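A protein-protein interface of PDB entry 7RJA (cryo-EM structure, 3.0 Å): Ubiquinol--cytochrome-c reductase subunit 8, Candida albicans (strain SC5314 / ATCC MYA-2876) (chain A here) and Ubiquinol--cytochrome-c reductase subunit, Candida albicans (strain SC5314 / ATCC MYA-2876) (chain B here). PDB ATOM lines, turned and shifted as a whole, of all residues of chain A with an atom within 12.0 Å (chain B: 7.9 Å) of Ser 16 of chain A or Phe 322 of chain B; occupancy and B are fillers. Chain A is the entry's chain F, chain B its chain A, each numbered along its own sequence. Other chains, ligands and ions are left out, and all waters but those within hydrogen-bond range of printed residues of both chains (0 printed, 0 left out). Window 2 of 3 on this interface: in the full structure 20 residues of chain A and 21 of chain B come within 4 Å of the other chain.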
ATOM      1  N   THR A   9      -2.153 -12.378  13.796  1.00  0.00           N
ATOM      2  CA  THR A   9      -1.484 -13.064  14.895  1.00  0.00           C
ATOM      3  C   THR A   9      -0.799 -12.066  15.815  1.00  0.00           C
ATOM      4  O   THR A   9      -0.708 -10.882  15.500  1.00  0.00           O
ATOM      5  CB  THR A   9      -0.439 -14.064  14.382  1.00  0.00           C
ATOM      6  OG1 THR A   9       0.721 -13.357  13.934  1.00  0.00           O
ATOM      7  CG2 THR A   9      -1.000 -14.883  13.237  1.00  0.00           C
ATOM      8  N   TYR A  10      -0.315 -12.555  16.957  1.00  0.00           N
ATOM      9  CA  TYR A  10       0.354 -11.726  17.951  1.00  0.00           C
ATOM     10  C   TYR A  10       1.849 -12.006  18.027  1.00  0.00           C
ATOM     11  O   TYR A  10       2.510 -11.571  18.974  1.00  0.00           O
ATOM     12  CB  TYR A  10      -0.292 -11.927  19.321  1.00  0.00           C
ATOM     13  CG  TYR A  10      -1.701 -11.392  19.427  1.00  0.00           C
ATOM     14  CD1 TYR A  10      -2.215 -10.519  18.482  1.00  0.00           C
ATOM     15  CD2 TYR A  10      -2.524 -11.773  20.470  1.00  0.00           C
ATOM     16  CE1 TYR A  10      -3.499 -10.034  18.583  1.00  0.00           C
ATOM     17  CE2 TYR A  10      -3.808 -11.297  20.577  1.00  0.00           C
ATOM     18  CZ  TYR A  10      -4.291 -10.429  19.632  1.00  0.00           C
ATOM     19  OH  TYR A  10      -5.575  -9.951  19.734  1.00  0.00           O
ATOM     20  N   MET A  11       2.398 -12.726  17.053  1.00  0.00           N
ATOM     21  CA  MET A  11       3.844 -12.907  16.973  1.00  0.00           C
ATOM     22  C   MET A  11       4.200 -13.153  15.515  1.00  0.00           C
ATOM     23  O   MET A  11       4.007 -14.264  15.014  1.00  0.00           O
ATOM     24  CB  MET A  11       4.304 -14.061  17.849  1.00  0.00           C
ATOM     25  CG  MET A  11       5.812 -14.263  17.835  1.00  0.00           C
ATOM     26  SD  MET A  11       6.326 -15.838  18.533  1.00  0.00           S
ATOM     27  CE  MET A  11       6.608 -16.789  17.045  1.00  0.00           C
ATOM     28  N   GLY A  12       4.717 -12.131  14.847  1.00  0.00           N
ATOM     29  CA  GLY A  12       5.220 -12.284  13.503  1.00  0.00           C
ATOM     30  C   GLY A  12       6.620 -12.857  13.515  1.00  0.00           C
ATOM     31  O   GLY A  12       7.134 -13.311  14.538  1.00  0.00           O
ATOM     32  N   TRP A  13       7.249 -12.835  12.348  1.00  0.00           N
ATOM     33  CA  TRP A  13       8.610 -13.336  12.229  1.00  0.00           C
ATOM     34  C   TRP A  13       9.581 -12.261  12.708  1.00  0.00           C
ATOM     35  O   TRP A  13       9.192 -11.259  13.312  1.00  0.00           O
ATOM     36  CB  TRP A  13       8.895 -13.782  10.800  1.00  0.00           C
ATOM     37  CG  TRP A  13       9.932 -14.859  10.729  1.00  0.00           C
ATOM     38  CD1 TRP A  13      11.085 -14.837  10.005  1.00  0.00           C
ATOM     39  CD2 TRP A  13       9.918 -16.110  11.422  1.00  0.00           C
ATOM     40  NE1 TRP A  13      11.788 -15.998  10.201  1.00  0.00           N
ATOM     41  CE2 TRP A  13      11.091 -16.797  11.068  1.00  0.00           C
ATOM     42  CE3 TRP A  13       9.025 -16.717  12.309  1.00  0.00           C
ATOM     43  CZ2 TRP A  13      11.394 -18.056  11.565  1.00  0.00           C
ATOM     44  CZ3 TRP A  13       9.327 -17.965  12.799  1.00  0.00           C
ATOM     45  CH2 TRP A  13      10.501 -18.622  12.428  1.00  0.00           C
ATOM     46  N   TRP A  14      10.870 -12.464  12.440  1.00  0.00           N
ATOM     47  CA  TRP A  14      11.893 -11.619  13.039  1.00  0.00           C
ATOM     48  C   TRP A  14      11.747 -10.166  12.607  1.00  0.00           C
ATOM     49  O   TRP A  14      11.889  -9.253  13.426  1.00  0.00           O
ATOM     50  CB  TRP A  14      13.271 -12.156  12.676  1.00  0.00           C
ATOM     51  CG  TRP A  14      13.684 -13.274  13.551  1.00  0.00           C
ATOM     52  CD1 TRP A  14      13.725 -14.594  13.228  1.00  0.00           C
ATOM     53  CD2 TRP A  14      14.113 -13.179  14.909  1.00  0.00           C
ATOM     54  NE1 TRP A  14      14.155 -15.328  14.302  1.00  0.00           N
ATOM     55  CE2 TRP A  14      14.400 -14.480  15.347  1.00  0.00           C
ATOM     56  CE3 TRP A  14      14.284 -12.116  15.796  1.00  0.00           C
ATOM     57  CZ2 TRP A  14      14.849 -14.747  16.630  1.00  0.00           C
ATOM     58  CZ3 TRP A  14      14.729 -12.383  17.067  1.00  0.00           C
ATOM     59  CH2 TRP A  14      15.006 -13.687  17.475  1.00  0.00           C
ATOM     60  N   GLY A  15      11.463  -9.928  11.330  1.00  0.00           N
ATOM     61  CA  GLY A  15      11.346  -8.558  10.868  1.00  0.00           C
ATOM     62  C   GLY A  15      10.294  -7.770  11.619  1.00  0.00           C
ATOM     63  O   GLY A  15      10.496  -6.593  11.924  1.00  0.00           O
ATOM     64  N   SER A  16       9.167  -8.404  11.934  1.00  0.00           N
ATOM     65  CA  SER A  16       8.076  -7.732  12.636  1.00  0.00           C
ATOM     66  C   SER A  16       7.514  -8.716  13.655  1.00  0.00           C
ATOM     67  O   SER A  16       6.639  -9.519  13.325  1.00  0.00           O
ATOM     68  CB  SER A  16       7.003  -7.269  11.662  1.00  0.00           C
ATOM     69  OG  SER A  16       6.366  -8.378  11.056  1.00  0.00           O
ATOM     70  N   LEU A  17       8.015  -8.643  14.884  1.00  0.00           N
ATOM     71  CA  LEU A  17       7.580  -9.528  15.953  1.00  0.00           C
ATOM     72  C   LEU A  17       6.348  -9.014  16.676  1.00  0.00           C
ATOM     73  O   LEU A  17       5.907  -9.645  17.641  1.00  0.00           O
ATOM     74  CB  LEU A  17       8.708  -9.726  16.966  1.00  0.00           C
ATOM     75  CG  LEU A  17       9.930 -10.504  16.490  1.00  0.00           C
ATOM     76  CD1 LEU A  17      11.055 -10.370  17.490  1.00  0.00           C
ATOM     77  CD2 LEU A  17       9.575 -11.958  16.287  1.00  0.00           C
ATOM     78  N   GLY A  18       5.786  -7.891  16.244  1.00  0.00           N
ATOM     79  CA  GLY A  18       4.675  -7.289  16.942  1.00  0.00           C
ATOM     80  C   GLY A  18       5.067  -6.417  18.110  1.00  0.00           C
ATOM     81  O   GLY A  18       4.180  -5.864  18.772  1.00  0.00           O
ATOM     82  N   SER A  19       6.355  -6.278  18.389  1.00  0.00           N
ATOM     83  CA  SER A  19       6.781  -5.380  19.444  1.00  0.00           C
ATOM     84  C   SER A  19       6.429  -3.944  19.068  1.00  0.00           C
ATOM     85  O   SER A  19       6.550  -3.565  17.899  1.00  0.00           O
ATOM     86  CB  SER A  19       8.284  -5.500  19.672  1.00  0.00           C
ATOM     87  OG  SER A  19       8.977  -5.516  18.438  1.00  0.00           O
ATOM     88  N   PRO A  20       5.992  -3.123  20.019  1.00  0.00           N
ATOM     89  CA  PRO A  20       5.714  -1.721  19.697  1.00  0.00           C
ATOM     90  C   PRO A  20       6.970  -1.036  19.187  1.00  0.00           C
ATOM     91  O   PRO A  20       8.080  -1.563  19.275  1.00  0.00           O
ATOM     92  CB  PRO A  20       5.244  -1.127  21.028  1.00  0.00           C
ATOM     93  CG  PRO A  20       4.902  -2.292  21.884  1.00  0.00           C
ATOM     94  CD  PRO A  20       5.796  -3.399  21.451  1.00  0.00           C
ATOM     95  N   LYS A  21       6.786   0.156  18.632  1.00  0.00           N
ATOM     96  CA  LYS A  21       7.935   0.934  18.190  1.00  0.00           C
ATOM     97  C   LYS A  21       8.912   1.082  19.340  1.00  0.00           C
ATOM     98  O   LYS A  21       8.599   1.711  20.355  1.00  0.00           O
ATOM     99  CB  LYS A  21       7.487   2.309  17.695  1.00  0.00           C
ATOM    100  CG  LYS A  21       6.548   2.280  16.507  1.00  0.00           C
ATOM    101  CD  LYS A  21       7.248   1.798  15.254  1.00  0.00           C
ATOM    102  CE  LYS A  21       6.296   1.771  14.077  1.00  0.00           C
ATOM    103  NZ  LYS A  21       5.898   3.149  13.683  1.00  0.00           N
ATOM    104  N   GLN A  22      10.094   0.495  19.190  1.00  0.00           N
ATOM    105  CA  GLN A  22      11.115   0.518  20.224  1.00  0.00           C
ATOM    106  C   GLN A  22      12.223   1.457  19.780  1.00  0.00           C
ATOM    107  O   GLN A  22      12.576   1.490  18.598  1.00  0.00           O
ATOM    108  CB  GLN A  22      11.653  -0.890  20.505  1.00  0.00           C
ATOM    109  CG  GLN A  22      12.777  -0.929  21.531  1.00  0.00           C
ATOM    110  CD  GLN A  22      13.419  -2.296  21.656  1.00  0.00           C
ATOM    111  OE1 GLN A  22      12.943  -3.270  21.083  1.00  0.00           O
ATOM    112  NE2 GLN A  22      14.513  -2.371  22.404  1.00  0.00           N
ATOM    113  N   ALA B 243      18.025  -0.371   7.911  1.00  0.00           N
ATOM    114  CA  ALA B 243      18.845  -0.951   8.964  1.00  0.00           C
ATOM    115  C   ALA B 243      20.300  -0.703   8.604  1.00  0.00           C
ATOM    116  O   ALA B 243      20.806  -1.267   7.631  1.00  0.00           O
ATOM    117  CB  ALA B 243      18.563  -2.441   9.129  1.00  0.00           C
ATOM    118  N   ILE B 295      18.805  -8.395  -1.230  1.00  0.00           N
ATOM    119  CA  ILE B 295      18.922  -8.539   0.217  1.00  0.00           C
ATOM    120  C   ILE B 295      19.279  -7.208   0.865  1.00  0.00           C
ATOM    121  O   ILE B 295      18.709  -6.832   1.894  1.00  0.00           O
ATOM    122  CB  ILE B 295      19.960  -9.624   0.558  1.00  0.00           C
ATOM    123  CG1 ILE B 295      19.565 -10.970  -0.053  1.00  0.00           C
ATOM    124  CG2 ILE B 295      20.114  -9.759   2.051  1.00  0.00           C
ATOM    125  CD1 ILE B 295      18.242 -11.523   0.438  1.00  0.00           C
ATOM    126  N   ILE B 318      20.460  -1.943   4.830  1.00  0.00           N
ATOM    127  CA  ILE B 318      19.460  -2.873   4.323  1.00  0.00           C
ATOM    128  C   ILE B 318      18.115  -2.166   4.324  1.00  0.00           C
ATOM    129  O   ILE B 318      17.677  -1.656   5.360  1.00  0.00           O
ATOM    130  CB  ILE B 318      19.402  -4.154   5.172  1.00  0.00           C
ATOM    131  CG1 ILE B 318      20.705  -4.940   5.052  1.00  0.00           C
ATOM    132  CG2 ILE B 318      18.228  -5.013   4.749  1.00  0.00           C
ATOM    133  CD1 ILE B 318      21.719  -4.601   6.106  1.00  0.00           C
ATOM    134  N   ALA B 319      17.455  -2.139   3.168  1.00  0.00           N
ATOM    135  CA  ALA B 319      16.158  -1.481   3.083  1.00  0.00           C
ATOM    136  C   ALA B 319      15.044  -2.390   3.586  1.00  0.00           C
ATOM    137  O   ALA B 319      14.173  -1.954   4.344  1.00  0.00           O
ATOM    138  CB  ALA B 319      15.884  -1.048   1.644  1.00  0.00           C
ATOM    139  N   ASP B 320      15.058  -3.655   3.175  1.00  0.00           N
ATOM    140  CA  ASP B 320      14.042  -4.613   3.597  1.00  0.00           C
ATOM    141  C   ASP B 320      14.389  -5.132   4.985  1.00  0.00           C
ATOM    142  O   ASP B 320      15.374  -5.854   5.156  1.00  0.00           O
ATOM    143  CB  ASP B 320      13.954  -5.756   2.591  1.00  0.00           C
ATOM    144  CG  ASP B 320      12.626  -6.487   2.648  1.00  0.00           C
ATOM    145  OD1 ASP B 320      11.678  -5.962   3.266  1.00  0.00           O
ATOM    146  OD2 ASP B 320      12.530  -7.588   2.068  1.00  0.00           O
ATOM    147  N   LYS B 321      13.574  -4.782   5.979  1.00  0.00           N
ATOM    148  CA  LYS B 321      13.886  -5.136   7.357  1.00  0.00           C
ATOM    149  C   LYS B 321      13.867  -6.637   7.605  1.00  0.00           C
ATOM    150  O   LYS B 321      14.348  -7.075   8.654  1.00  0.00           O
ATOM    151  CB  LYS B 321      12.904  -4.452   8.304  1.00  0.00           C
ATOM    152  CG  LYS B 321      11.468  -4.903   8.137  1.00  0.00           C
ATOM    153  CD  LYS B 321      10.543  -4.140   9.061  1.00  0.00           C
ATOM    154  CE  LYS B 321       9.108  -4.595   8.902  1.00  0.00           C
ATOM    155  NZ  LYS B 321       8.571  -4.256   7.559  1.00  0.00           N
ATOM    156  N   PHE B 322      13.327  -7.429   6.684  1.00  0.00           N
ATOM    157  CA  PHE B 322      13.237  -8.872   6.857  1.00  0.00           C
ATOM    158  C   PHE B 322      14.461  -9.617   6.348  1.00  0.00           C
ATOM    159  O   PHE B 322      14.488 -10.848   6.425  1.00  0.00           O
ATOM    160  CB  PHE B 322      11.999  -9.413   6.139  1.00  0.00           C
ATOM    161  CG  PHE B 322      10.708  -8.945   6.728  1.00  0.00           C
ATOM    162  CD1 PHE B 322      10.129  -7.767   6.307  1.00  0.00           C
ATOM    163  CD2 PHE B 322      10.070  -9.689   7.697  1.00  0.00           C
ATOM    164  CE1 PHE B 322       8.943  -7.336   6.847  1.00  0.00           C
ATOM    165  CE2 PHE B 322       8.882  -9.264   8.241  1.00  0.00           C
ATOM    166  CZ  PHE B 322       8.317  -8.086   7.817  1.00  0.00           C
ATOM    167  N   THR B 323      15.470  -8.914   5.832  1.00  0.00           N
ATOM    168  CA  THR B 323      16.608  -9.571   5.203  1.00  0.00           C
ATOM    169  C   THR B 323      17.937  -9.157   5.821  1.00  0.00           C
ATOM    170  O   THR B 323      18.984  -9.343   5.198  1.00  0.00           O
ATOM    171  CB  THR B 323      16.625  -9.286   3.702  1.00  0.00           C
ATOM    172  OG1 THR B 323      16.989  -7.920   3.479  1.00  0.00           O
ATOM    173  CG2 THR B 323      15.260  -9.546   3.100  1.00  0.00           C
ATOM    174  N   VAL B 324      17.926  -8.600   7.031  1.00  0.00           N
ATOM    175  CA  VAL B 324      19.185  -8.288   7.698  1.00  0.00           C
ATOM    176  C   VAL B 324      19.951  -9.567   8.002  1.00  0.00           C
ATOM    177  O   VAL B 324      21.166  -9.652   7.780  1.00  0.00           O
ATOM    178  CB  VAL B 324      18.930  -7.467   8.972  1.00  0.00           C
ATOM    179  CG1 VAL B 324      20.238  -6.965   9.544  1.00  0.00           C
ATOM    180  CG2 VAL B 324      18.003  -6.303   8.677  1.00  0.00           C
ATOM    181  N   ASP B 325      19.253 -10.584   8.507  1.00  0.00           N
ATOM    182  CA  ASP B 325      19.915 -11.843   8.823  1.00  0.00           C
ATOM    183  C   ASP B 325      20.494 -12.487   7.574  1.00  0.00           C
ATOM    184  O   ASP B 325      21.602 -13.029   7.605  1.00  0.00           O
ATOM    185  CB  ASP B 325      18.940 -12.800   9.498  1.00  0.00           C
ATOM    186  CG  ASP B 325      19.563 -14.148   9.785  1.00  0.00           C
ATOM    187  OD1 ASP B 325      20.758 -14.181  10.147  1.00  0.00           O
ATOM    188  OD2 ASP B 325      18.866 -15.173   9.642  1.00  0.00           O
ATOM    189  N   ASP B 326      19.751 -12.454   6.466  1.00  0.00           N
ATOM    190  CA  ASP B 326      20.264 -13.035   5.232  1.00  0.00           C
ATOM    191  C   ASP B 326      21.533 -12.330   4.783  1.00  0.00           C
ATOM    192  O   ASP B 326      22.502 -12.981   4.371  1.00  0.00           O
ATOM    193  CB  ASP B 326      19.201 -12.971   4.139  1.00  0.00           C
ATOM    194  CG  ASP B 326      17.939 -13.713   4.515  1.00  0.00           C
ATOM    195  OD1 ASP B 326      17.950 -14.414   5.546  1.00  0.00           O
ATOM    196  OD2 ASP B 326      16.937 -13.599   3.778  1.00  0.00           O
ATOM    197  N   PHE B 327      21.554 -10.999   4.854  1.00  0.00           N
ATOM    198  CA  PHE B 327      22.756 -10.278   4.455  1.00  0.00           C
ATOM    199  C   PHE B 327      23.930 -10.628   5.350  1.00  0.00           C
ATOM    200  O   PHE B 327      25.044 -10.845   4.867  1.00  0.00           O
ATOM    201  CB  PHE B 327      22.542  -8.774   4.483  1.00  0.00           C
ATOM    202  CG  PHE B 327      23.765  -8.014   4.095  1.00  0.00           C
ATOM    203  CD1 PHE B 327      24.248  -8.077   2.804  1.00  0.00           C
ATOM    204  CD2 PHE B 327      24.463  -7.276   5.027  1.00  0.00           C
ATOM    205  CE1 PHE B 327      25.383  -7.396   2.445  1.00  0.00           C
ATOM    206  CE2 PHE B 327      25.600  -6.595   4.671  1.00  0.00           C
ATOM    207  CZ  PHE B 327      26.061  -6.656   3.380  1.00  0.00           C
ATOM    208  N   LEU B 420      15.568  -0.744  12.678  1.00  0.00           N
ATOM    209  CA  LEU B 420      14.933  -1.915  12.082  1.00  0.00           C
ATOM    210  C   LEU B 420      15.864  -3.122  12.129  1.00  0.00           C
ATOM    211  O   LEU B 420      15.931  -3.923  11.196  1.00  0.00           O
ATOM    212  CB  LEU B 420      14.494  -1.617  10.648  1.00  0.00           C
ATOM    213  CG  LEU B 420      13.153  -0.896  10.514  1.00  0.00           C
ATOM    214  CD1 LEU B 420      13.239   0.503  11.072  1.00  0.00           C
ATOM    215  CD2 LEU B 420      12.715  -0.858   9.065  1.00  0.00           C
ATOM    216  N   GLU B 422      15.593  -5.564  14.241  1.00  0.00           N
ATOM    217  CA  GLU B 422      14.948  -6.708  14.871  1.00  0.00           C
ATOM    218  C   GLU B 422      15.401  -8.013  14.242  1.00  0.00           C
ATOM    219  O   GLU B 422      15.507  -9.030  14.935  1.00  0.00           O
ATOM    220  CB  GLU B 422      13.432  -6.576  14.768  1.00  0.00           C
ATOM    221  CG  GLU B 422      12.666  -7.449  15.740  1.00  0.00           C
ATOM    222  CD  GLU B 422      11.190  -7.113  15.775  1.00  0.00           C
ATOM    223  OE1 GLU B 422      10.466  -7.509  14.839  1.00  0.00           O
ATOM    224  OE2 GLU B 422      10.756  -6.441  16.734  1.00  0.00           O
ATOM    225  N   ASP B 423      15.675  -8.011  12.940  1.00  0.00           N
ATOM    226  CA  ASP B 423      16.090  -9.229  12.264  1.00  0.00           C
ATOM    227  C   ASP B 423      17.574  -9.520  12.413  1.00  0.00           C
ATOM    228  O   ASP B 423      18.014 -10.604  12.022  1.00  0.00           O
ATOM    229  CB  ASP B 423      15.744  -9.158  10.780  1.00  0.00           C
ATOM    230  CG  ASP B 423      15.766 -10.517  10.119  1.00  0.00           C
ATOM    231  OD1 ASP B 423      14.788 -11.273  10.284  1.00  0.00           O
ATOM    232  OD2 ASP B 423      16.765 -10.836   9.445  1.00  0.00           O
ATOM    233  N   LEU B 424      18.356  -8.594  12.956  1.00  0.00           N
ATOM    234  CA  LEU B 424      19.772  -8.848  13.200  1.00  0.00           C
ATOM    235  C   LEU B 424      19.887  -9.807  14.374  1.00  0.00           C
ATOM    236  O   LEU B 424      19.794  -9.403  15.535  1.00  0.00           O
ATOM    237  CB  LEU B 424      20.511  -7.545  13.476  1.00  0.00           C
ATOM    238  CG  LEU B 424      22.004  -7.681  13.771  1.00  0.00           C
ATOM    239  CD1 LEU B 424      22.740  -8.186  12.552  1.00  0.00           C
ATOM    240  CD2 LEU B 424      22.582  -6.359  14.230  1.00  0.00           C
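OE1 of Glu 422 of chain B lies close to O of Trp 14 of chain A, 2.7 Å away. The backbone NH of Ser 16 of chain A sits close to the side-chain carboxylate of Glu 422 of chain B, at 3.3 Å. The backbone NH (N) of Leu 17 of chain A sits at hydrogen-bond distance from the side-chain carboxylate (OE1) of Glu 422 of chain B, 2.7 Å away. The side-chain hydroxyl of Ser 19 of chain A lies within hydrogen-bond range of the side-chain carboxylate of Glu 422 of chain B (2.6 Å). O of Gly 15 of chain A sits close to OE1 of Glu 422 of chain B (3.1 Å).
The backbone NH of Val 324 of chain B is in hydrogen-bond range of the side-chain carboxylate of Asp 423 of chain B. The side-chain carboxylate (OD2) of Asp 423 of chain B sits at hydrogen-bond distance from the backbone NH (N) of Asp 325 of chain B, at 2.7 Å.
Trp 14 of chain A touches Asp 423 of chain B. Gly 15 of chain A touches Lys 321 of chain B. Phe 322 of chain B touches Gly 15 of chain A (CD2 to CA, 3.6 Å). Gly 15 of chain A touches Asp 423 of chain B. CZ of Phe 322 of chain B touches OG of Ser 16 of chain A (3.8 Å).
Of chain B, only Phe 322 and Glu 422 come within 4 Å of Ser 16 of chain A. Phe 322 of chain B touches just these residues of chain A: Gly 15 and Ser 16. Of chain B, only Lys 321 (3.8 Å), Phe 322 (3.6 Å), Glu 422 (3.1 Å) and Asp 423 (3.7 Å) come within 4 Å of Gly 15 of chain A. No residue of chain A comes within 4 Å of Asp 320 of chain B. Lys 321 of chain B touches just one residue of chain A: Gly 15. No residue of chain A comes within 4 Å of Val 324 of chain B. Of chain A, only Trp 14 (2.7 Å), Gly 15 (3.1 Å), Ser 16 (3.3 Å), Leu 17 (2.7 Å) and Ser 19 (2.6 Å) come within 4 Å of Glu 422 of chain B. Of the printed residues of chain B, Ser 19 of chain A touches Glu 422 (2.6 Å). Of the printed residues of chain B, Leu 17 of chain A touches Glu 422 (2.7 Å). Printed residues of chain B within 4 Å of Trp 14 of chain A: Glu 422 (2.7 Å) and Asp 423 (3.0 Å). The nearest residue of chain B that does not touch Ser 16 of chain A is Lys 321 of chain B (4.4 Å).
Printed residues of chain B that touch a printed residue of chain A: Lys 321, Phe 322, Glu 422 and Asp 423. Printed residues of chain A that touch a printed residue of chain B: Trp 14, Gly 15, Ser 16, Leu 17 and Ser 19. Hydrophobic or aromatic side chains of chain A within 4 Å of the printed part of chain B: Trp 14 and Leu 17. Along chain A the printed residues that touch a printed residue of chain B span positions 14 to 19. Among the printed residues, no Asp or Glu carboxylate lies within 4 Å of a Lys or Arg side-chain nitrogen of the other chain.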
